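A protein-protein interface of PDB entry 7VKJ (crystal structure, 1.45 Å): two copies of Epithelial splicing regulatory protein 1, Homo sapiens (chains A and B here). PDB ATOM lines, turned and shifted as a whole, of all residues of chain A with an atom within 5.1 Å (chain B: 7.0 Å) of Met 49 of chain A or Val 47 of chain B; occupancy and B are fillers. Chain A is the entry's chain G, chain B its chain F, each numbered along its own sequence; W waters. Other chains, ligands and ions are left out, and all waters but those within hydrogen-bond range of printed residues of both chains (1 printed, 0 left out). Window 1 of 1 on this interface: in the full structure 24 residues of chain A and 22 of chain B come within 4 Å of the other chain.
N of Gly 46 of chain B sits at hydrogen-bond distance from OG1 of Thr 44 of chain B.
O of His 48 of chain B sits at hydrogen-bond distance from N of Phe 62 of chain B.
The backbone carbonyl oxygen (O) of Asp 60 of chain A is in hydrogen-bond range of the backbone NH (N) of Val 50 of chain A.
Of the 9 printed residues of chain A, 5 touch a printed residue of chain B.
Hydrophobic or aromatic side chains of chain A that line the printed part of chain B: His 48, Met 49, Val 50 and Leu 51.
Of the 17 printed residues of chain B, 6 touch a printed residue of chain A.
Among the printed residues, merely in contact across the chains: Met 49 of chain A with Gly 46 of chain B (3.3 Å), Val 50 of chain A with His 45 of chain B (3.3 Å), Val 47 of chain A with His 48 of chain B (3.6 Å), His 48 of chain A with Val 47 of chain B (3.6 Å), His 48 of chain A with His 48 of chain B (3.7 Å), Met 49 of chain A with Met 49 of chain B (3.8 Å), Met 49 of chain A with His 45 of chain B (3.9 Å) and Leu 51 of chain A with Ile 42 of chain B (3.98 Å).
Val 47 of chain B touches its own counterpart, Val 47 of chain A.
Val 47 of chain A touches His 48 of chain B, and with the chains exchanged His 48 of chain A touches Val 47 of chain B.
His 48 of chain A touches its own counterpart, His 48 of chain B.
Met 49 of chain B touches its own counterpart, Met 49 of chain A.
The backbone carbonyl oxygen (O) of His 45 of chain B is in hydrogen-bond range of the backbone NH (N) of Leu 51 of chain A (2.8 Å).
The backbone carbonyl oxygen (O) of Val 47 of chain B is in hydrogen-bond range of the backbone NH (N) of Met 49 of chain A, at 2.9 Å.
The backbone NH (N) of Met 49 of chain B is in hydrogen-bond range of the backbone carbonyl oxygen (O) of Val 47 of chain A (2.8 Å).
The backbone carbonyl oxygen (O) of Val 47 of chain A lies close to the backbone carbonyl oxygen (O) of Val 47 of chain B (3.5 Å).
Water W1 lies within hydrogen-bond range of a ring nitrogen (ND1) of His 48 of chain B, a ring nitrogen (NE2) of His 48 of chain A and the backbone NH of Val 47 of chain A.
Of the printed residues of chain B, His 48 of chain A touches Val 47 and His 48.
Printed residues of chain B within 4 Å of Met 49 of chain A: His 45, Gly 46, Val 47 and Met 49.
Of the printed residues of chain B, Leu 51 of chain A touches Ile 42 (3.98 Å) and His 45 (2.8 Å).
Of the printed residues of chain A, Ile 42 of chain B touches Leu 51.
Of chain A, only Val 47, His 48 and Met 49 come within 4 Å of Val 47 of chain B.
Of the printed residues of chain A, His 48 of chain B touches Val 47 and His 48.
Of the printed residues of chain A, Met 49 of chain B touches Val 47 and Met 49.
Ile 63 of chain B touches none of the printed residues of chain A.
The nearest residue of chain A that does not touch Val 47 of chain B is Leu 51 of chain A (4.2 Å).
The nearest printed residue of chain B that does not touch Val 47 of chain A is Gly 46 of chain B (7.1 Å).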
ATOM      1  N   LEU A  22      10.236 -14.090  19.357  1.00  0.00           N
ATOM      2  CA  LEU A  22      10.613 -12.695  19.135  1.00  0.00           C
ATOM      3  C   LEU A  22       9.381 -11.852  18.823  1.00  0.00           C
ATOM      4  O   LEU A  22       8.489 -12.260  18.076  1.00  0.00           O
ATOM      5  CB  LEU A  22      11.599 -12.588  17.974  1.00  0.00           C
ATOM      6  CG  LEU A  22      12.991 -13.110  18.269  1.00  0.00           C
ATOM      7  CD1 LEU A  22      13.751 -13.244  16.960  1.00  0.00           C
ATOM      8  CD2 LEU A  22      13.719 -12.229  19.241  1.00  0.00           C
ATOM      9  N   ILE A  31      17.608  -7.121  19.478  1.00  0.00           N
ATOM     10  CA  ILE A  31      18.271  -8.397  19.826  1.00  0.00           C
ATOM     11  C   ILE A  31      19.608  -8.107  20.506  1.00  0.00           C
ATOM     12  O   ILE A  31      19.904  -8.767  21.535  1.00  0.00           O
ATOM     13  CB  ILE A  31      18.452  -9.238  18.550  1.00  0.00           C
ATOM     14  CG1 ILE A  31      17.072  -9.672  18.059  1.00  0.00           C
ATOM     15  CG2 ILE A  31      19.380 -10.401  18.832  1.00  0.00           C
ATOM     16  CD1 ILE A  31      17.087 -10.333  16.673  1.00  0.00           C
ATOM     17  N   VAL A  47      23.347 -12.753  12.468  1.00  0.00           N
ATOM     18  CA  VAL A  47      22.195 -13.277  13.254  1.00  0.00           C
ATOM     19  C   VAL A  47      21.213 -13.849  12.262  1.00  0.00           C
ATOM     20  O   VAL A  47      20.788 -13.156  11.296  1.00  0.00           O
ATOM     21  CB  VAL A  47      21.534 -12.195  14.129  1.00  0.00           C
ATOM     22  CG1 VAL A  47      20.235 -12.685  14.738  1.00  0.00           C
ATOM     23  CG2 VAL A  47      22.562 -11.764  15.169  1.00  0.00           C
ATOM     24  N   HIS A  48      20.819 -15.092  12.436  1.00  0.00           N
ATOM     25  CA  HIS A  48      19.909 -15.750  11.492  1.00  0.00           C
ATOM     26  C   HIS A  48      18.462 -15.581  11.929  1.00  0.00           C
ATOM     27  O   HIS A  48      18.066 -16.126  12.983  1.00  0.00           O
ATOM     28  CB  HIS A  48      20.148 -17.250  11.432  1.00  0.00           C
ATOM     29  CG  HIS A  48      21.493 -17.685  11.124  1.00  0.00           C
ATOM     30  ND1 HIS A  48      21.805 -18.106   9.842  1.00  0.00           N
ATOM     31  CD2 HIS A  48      22.552 -17.903  11.921  1.00  0.00           C
ATOM     32  CE1 HIS A  48      23.055 -18.541   9.873  1.00  0.00           C
ATOM     33  NE2 HIS A  48      23.539 -18.425  11.157  1.00  0.00           N
ATOM     34  N   MET A  49      17.661 -14.889  11.184  1.00  0.00           N
ATOM     35  CA  MET A  49      16.213 -14.776  11.398  1.00  0.00           C
ATOM     36  C   MET A  49      15.525 -15.902  10.669  1.00  0.00           C
ATOM     37  O   MET A  49      15.699 -16.044   9.471  1.00  0.00           O
ATOM     38  CB  MET A  49      15.645 -13.431  10.948  1.00  0.00           C
ATOM     39  CG  MET A  49      16.319 -12.247  11.630  1.00  0.00           C
ATOM     40  SD  MET A  49      15.970 -12.157  13.404  1.00  0.00           S
ATOM     41  CE  MET A  49      14.229 -11.753  13.360  1.00  0.00           C
ATOM     42  N   VAL A  50      14.737 -16.701  11.354  1.00  0.00           N
ATOM     43  CA  VAL A  50      14.189 -17.946  10.809  1.00  0.00           C
ATOM     44  C   VAL A  50      12.819 -17.742  10.165  1.00  0.00           C
ATOM     45  O   VAL A  50      11.962 -16.982  10.666  1.00  0.00           O
ATOM     46  CB  VAL A  50      14.149 -19.000  11.924  1.00  0.00           C
ATOM     47  CG1 VAL A  50      13.537 -20.284  11.404  1.00  0.00           C
ATOM     48  CG2 VAL A  50      15.525 -19.252  12.527  1.00  0.00           C
ATOM     49  N   LEU A  51      12.628 -18.372   9.019  1.00  0.00           N
ATOM     50  CA  LEU A  51      11.351 -18.428   8.271  1.00  0.00           C
ATOM     51  C   LEU A  51      10.672 -19.795   8.452  1.00  0.00           C
ATOM     52  O   LEU A  51      11.379 -20.792   8.694  1.00  0.00           O
ATOM     53  CB  LEU A  51      11.622 -18.136   6.782  1.00  0.00           C
ATOM     54  CG  LEU A  51      12.364 -16.847   6.490  1.00  0.00           C
ATOM     55  CD1 LEU A  51      12.614 -16.740   4.990  1.00  0.00           C
ATOM     56  CD2 LEU A  51      11.658 -15.626   7.015  1.00  0.00           C
ATOM     57  N   ASP A  60      11.640 -17.283  15.545  1.00  0.00           N
ATOM     58  CA  ASP A  60      12.935 -17.818  16.044  1.00  0.00           C
ATOM     59  C   ASP A  60      14.086 -17.029  15.387  1.00  0.00           C
ATOM     60  O   ASP A  60      13.982 -16.527  14.251  1.00  0.00           O
ATOM     61  CB  ASP A  60      13.097 -19.309  15.773  1.00  0.00           C
ATOM     62  CG  ASP A  60      12.276 -20.309  16.599  1.00  0.00           C
ATOM     63  OD1 ASP A  60      11.610 -19.890  17.512  1.00  0.00           O
ATOM     64  OD2 ASP A  60      12.344 -21.532  16.273  1.00  0.00           O
ATOM     65  N   ALA A  61      15.217 -17.018  16.078  1.00  0.00           N
ATOM     66  CA  ALA A  61      16.507 -16.610  15.532  1.00  0.00           C
ATOM     67  C   ALA A  61      17.565 -17.531  16.086  1.00  0.00           C
ATOM     68  O   ALA A  61      17.444 -18.042  17.230  1.00  0.00           O
ATOM     69  CB  ALA A  61      16.814 -15.161  15.862  1.00  0.00           C
ATOM     70  N   LEU B  19      20.882  -6.504   1.097  1.00  0.00           N
ATOM     71  CA  LEU B  19      20.151  -5.253   1.369  1.00  0.00           C
ATOM     72  C   LEU B  19      21.104  -4.376   2.178  1.00  0.00           C
ATOM     73  O   LEU B  19      21.768  -4.843   3.099  1.00  0.00           O
ATOM     74  CB  LEU B  19      18.831  -5.506   2.100  1.00  0.00           C
ATOM     75  CG  LEU B  19      17.890  -6.534   1.485  1.00  0.00           C
ATOM     76  CD1 LEU B  19      16.598  -6.588   2.295  1.00  0.00           C
ATOM     77  CD2 LEU B  19      17.539  -6.218   0.091  1.00  0.00           C
ATOM     78  N   THR B  27      12.022  -4.613  10.370  1.00  0.00           N
ATOM     79  CA  THR B  27      11.790  -5.973  10.887  1.00  0.00           C
ATOM     80  C   THR B  27      11.885  -7.011   9.775  1.00  0.00           C
ATOM     81  O   THR B  27      11.938  -6.654   8.599  1.00  0.00           O
ATOM     82  CB  THR B  27      10.408  -6.043  11.526  1.00  0.00           C
ATOM     83  OG1 THR B  27       9.457  -5.997  10.464  1.00  0.00           O
ATOM     84  CG2 THR B  27      10.205  -4.907  12.513  1.00  0.00           C
ATOM     85  N   ILE B  28      11.894  -8.280  10.164  1.00  0.00           N
ATOM     86  CA  ILE B  28      11.882  -9.344   9.133  1.00  0.00           C
ATOM     87  C   ILE B  28      10.582  -9.264   8.329  1.00  0.00           C
ATOM     88  O   ILE B  28      10.636  -9.448   7.101  1.00  0.00           O
ATOM     89  CB  ILE B  28      12.160 -10.715   9.757  1.00  0.00           C
ATOM     90  CG1 ILE B  28      12.242 -11.784   8.670  1.00  0.00           C
ATOM     91  CG2 ILE B  28      11.175 -11.150  10.845  1.00  0.00           C
ATOM     92  CD1 ILE B  28      13.428 -11.613   7.771  1.00  0.00           C
ATOM     93  N   ILE B  31      11.190  -6.641   5.672  1.00  0.00           N
ATOM     94  CA  ILE B  31      12.141  -7.100   4.621  1.00  0.00           C
ATOM     95  C   ILE B  31      11.317  -7.924   3.633  1.00  0.00           C
ATOM     96  O   ILE B  31      11.458  -7.736   2.392  1.00  0.00           O
ATOM     97  CB  ILE B  31      13.335  -7.840   5.242  1.00  0.00           C
ATOM     98  CG1 ILE B  31      14.280  -6.843   5.943  1.00  0.00           C
ATOM     99  CG2 ILE B  31      14.052  -8.624   4.166  1.00  0.00           C
ATOM    100  CD1 ILE B  31      15.347  -7.477   6.783  1.00  0.00           C
ATOM    101  N   LEU B  32      10.493  -8.832   4.150  1.00  0.00           N
ATOM    102  CA  LEU B  32       9.731  -9.721   3.235  1.00  0.00           C
ATOM    103  C   LEU B  32       8.737  -8.889   2.442  1.00  0.00           C
ATOM    104  O   LEU B  32       8.559  -9.144   1.235  1.00  0.00           O
ATOM    105  CB  LEU B  32       9.018 -10.801   4.039  1.00  0.00           C
ATOM    106  CG  LEU B  32       9.900 -11.804   4.742  1.00  0.00           C
ATOM    107  CD1 LEU B  32       9.087 -12.757   5.627  1.00  0.00           C
ATOM    108  CD2 LEU B  32      10.749 -12.585   3.767  1.00  0.00           C
ATOM    109  N   LEU B  35      10.414  -7.080  -0.480  1.00  0.00           N
ATOM    110  CA  LEU B  35      10.745  -7.942  -1.648  1.00  0.00           C
ATOM    111  C   LEU B  35       9.506  -8.223  -2.508  1.00  0.00           C
ATOM    112  O   LEU B  35       9.668  -8.636  -3.674  1.00  0.00           O
ATOM    113  CB  LEU B  35      11.391  -9.234  -1.157  1.00  0.00           C
ATOM    114  CG  LEU B  35      12.745  -9.064  -0.476  1.00  0.00           C
ATOM    115  CD1 LEU B  35      13.155 -10.407   0.112  1.00  0.00           C
ATOM    116  CD2 LEU B  35      13.799  -8.495  -1.424  1.00  0.00           C
ATOM    117  N   ILE B  42      12.885 -16.730  -2.075  1.00  0.00           N
ATOM    118  CA  ILE B  42      13.908 -16.994  -1.021  1.00  0.00           C
ATOM    119  C   ILE B  42      14.167 -18.494  -0.909  1.00  0.00           C
ATOM    120  O   ILE B  42      13.201 -19.284  -0.941  1.00  0.00           O
ATOM    121  CB  ILE B  42      13.478 -16.370   0.330  1.00  0.00           C
ATOM    122  CG1 ILE B  42      13.393 -14.856   0.178  1.00  0.00           C
ATOM    123  CG2 ILE B  42      14.406 -16.812   1.442  1.00  0.00           C
ATOM    124  CD1 ILE B  42      12.857 -14.166   1.417  1.00  0.00           C
ATOM    125  N   THR B  44      16.387 -20.737   1.500  1.00  0.00           N
ATOM    126  CA  THR B  44      16.523 -21.427   2.794  1.00  0.00           C
ATOM    127  C   THR B  44      15.422 -20.918   3.750  1.00  0.00           C
ATOM    128  O   THR B  44      14.512 -20.126   3.360  1.00  0.00           O
ATOM    129  CB  THR B  44      17.908 -21.184   3.403  1.00  0.00           C
ATOM    130  OG1 THR B  44      17.934 -19.841   3.866  1.00  0.00           O
ATOM    131  CG2 THR B  44      19.077 -21.383   2.453  1.00  0.00           C
ATOM    132  N   HIS B  45      15.517 -21.326   4.997  1.00  0.00           N
ATOM    133  CA  HIS B  45      14.582 -20.849   6.054  1.00  0.00           C
ATOM    134  C   HIS B  45      15.253 -19.772   6.900  1.00  0.00           C
ATOM    135  O   HIS B  45      14.933 -19.624   8.060  1.00  0.00           O
ATOM    136  CB  HIS B  45      14.106 -22.052   6.859  1.00  0.00           C
ATOM    137  CG  HIS B  45      13.083 -22.892   6.165  1.00  0.00           C
ATOM    138  ND1 HIS B  45      13.370 -23.688   5.071  1.00  0.00           N
ATOM    139  CD2 HIS B  45      11.769 -23.096   6.469  1.00  0.00           C
ATOM    140  CE1 HIS B  45      12.265 -24.308   4.693  1.00  0.00           C
ATOM    141  NE2 HIS B  45      11.266 -24.023   5.582  1.00  0.00           N
ATOM    142  N   GLY B  46      16.184 -19.022   6.349  1.00  0.00           N
ATOM    143  CA  GLY B  46      16.918 -18.004   7.116  1.00  0.00           C
ATOM    144  C   GLY B  46      17.211 -16.754   6.297  1.00  0.00           C
ATOM    145  O   GLY B  46      17.470 -16.836   5.065  1.00  0.00           O
ATOM    146  N   VAL B  47      17.164 -15.622   6.979  1.00  0.00           N
ATOM    147  CA  VAL B  47      17.650 -14.304   6.509  1.00  0.00           C
ATOM    148  C   VAL B  47      18.782 -13.872   7.427  1.00  0.00           C
ATOM    149  O   VAL B  47      18.638 -13.939   8.659  1.00  0.00           O
ATOM    150  CB  VAL B  47      16.522 -13.259   6.514  1.00  0.00           C
ATOM    151  CG1 VAL B  47      17.034 -11.848   6.251  1.00  0.00           C
ATOM    152  CG2 VAL B  47      15.465 -13.666   5.472  1.00  0.00           C
ATOM    153  N   HIS B  48      19.900 -13.409   6.914  1.00  0.00           N
ATOM    154  CA  HIS B  48      21.082 -13.052   7.731  1.00  0.00           C
ATOM    155  C   HIS B  48      21.105 -11.568   8.034  1.00  0.00           C
ATOM    156  O   HIS B  48      21.242 -10.755   7.093  1.00  0.00           O
ATOM    157  CB  HIS B  48      22.379 -13.419   7.062  1.00  0.00           C
ATOM    158  CG  HIS B  48      22.505 -14.798   6.587  1.00  0.00           C
ATOM    159  ND1 HIS B  48      23.116 -15.737   7.351  1.00  0.00           N
ATOM    160  CD2 HIS B  48      22.160 -15.372   5.416  1.00  0.00           C
ATOM    161  CE1 HIS B  48      23.224 -16.832   6.620  1.00  0.00           C
ATOM    162  NE2 HIS B  48      22.629 -16.620   5.420  1.00  0.00           N
ATOM    163  N   MET B  49      21.024 -11.168   9.278  1.00  0.00           N
ATOM    164  CA  MET B  49      21.235  -9.746   9.645  1.00  0.00           C
ATOM    165  C   MET B  49      22.693  -9.577   9.990  1.00  0.00           C
ATOM    166  O   MET B  49      23.264 -10.352  10.783  1.00  0.00           O
ATOM    167  CB  MET B  49      20.397  -9.347  10.851  1.00  0.00           C
ATOM    168  CG  MET B  49      18.993  -9.744  10.755  1.00  0.00           C
ATOM    169  SD  MET B  49      18.117  -9.171   9.371  1.00  0.00           S
ATOM    170  CE  MET B  49      18.116  -7.424   9.715  1.00  0.00           C
ATOM    171  N   ALA B  61      21.679  -6.837   5.279  1.00  0.00           N
ATOM    172  CA  ALA B  61      21.150  -8.207   5.384  1.00  0.00           C
ATOM    173  C   ALA B  61      21.515  -8.965   4.127  1.00  0.00           C
ATOM    174  O   ALA B  61      21.626  -8.330   3.037  1.00  0.00           O
ATOM    175  CB  ALA B  61      19.675  -8.176   5.594  1.00  0.00           C
ATOM    176  N   PHE B  62      21.639 -10.277   4.241  1.00  0.00           N
ATOM    177  CA  PHE B  62      21.847 -11.152   3.076  1.00  0.00           C
ATOM    178  C   PHE B  62      20.701 -12.154   3.016  1.00  0.00           C
ATOM    179  O   PHE B  62      20.278 -12.716   4.034  1.00  0.00           O
ATOM    180  CB  PHE B  62      23.162 -11.917   3.091  1.00  0.00           C
ATOM    181  CG  PHE B  62      24.390 -11.093   2.831  1.00  0.00           C
ATOM    182  CD1 PHE B  62      24.845 -10.911   1.542  1.00  0.00           C
ATOM    183  CD2 PHE B  62      25.142 -10.574   3.875  1.00  0.00           C
ATOM    184  CE1 PHE B  62      26.019 -10.214   1.282  1.00  0.00           C
ATOM    185  CE2 PHE B  62      26.295  -9.851   3.601  1.00  0.00           C
ATOM    186  CZ  PHE B  62      26.732  -9.674   2.315  1.00  0.00           C
ATOM    187  N   ILE B  63      20.257 -12.411   1.809  1.00  0.00           N
ATOM    188  CA  ILE B  63      19.212 -13.425   1.507  1.00  0.00           C
ATOM    189  C   ILE B  63      19.646 -14.260   0.326  1.00  0.00           C
ATOM    190  O   ILE B  63      20.013 -13.693  -0.741  1.00  0.00           O
ATOM    191  CB  ILE B  63      17.897 -12.721   1.220  1.00  0.00           C
ATOM    192  CG1 ILE B  63      17.532 -11.738   2.322  1.00  0.00           C
ATOM    193  CG2 ILE B  63      16.788 -13.739   0.996  1.00  0.00           C
ATOM    194  CD1 ILE B  63      16.269 -11.034   2.099  1.00  0.00           C
ATOM    195  N   GLN B  64      19.616 -15.575   0.476  1.00  0.00           N
ATOM    196  CA  GLN B  64      19.883 -16.480  -0.630  1.00  0.00           C
ATOM    197  C   GLN B  64      18.575 -16.738  -1.374  1.00  0.00           C
ATOM    198  O   GLN B  64      17.572 -17.016  -0.761  1.00  0.00           O
ATOM    199  CB  GLN B  64      20.526 -17.792  -0.213  1.00  0.00           C
ATOM    200  CG  GLN B  64      20.993 -18.530  -1.468  1.00  0.00           C
ATOM    201  CD  GLN B  64      21.906 -19.687  -1.228  1.00  0.00           C
ATOM    202  OE1 GLN B  64      21.649 -20.483  -0.340  1.00  0.00           O
ATOM    203  NE2 GLN B  64      22.860 -19.877  -2.120  1.00  0.00           N
HETATM  204  O   HOH W   1      23.786 -15.268  10.176  1.00  0.00           O
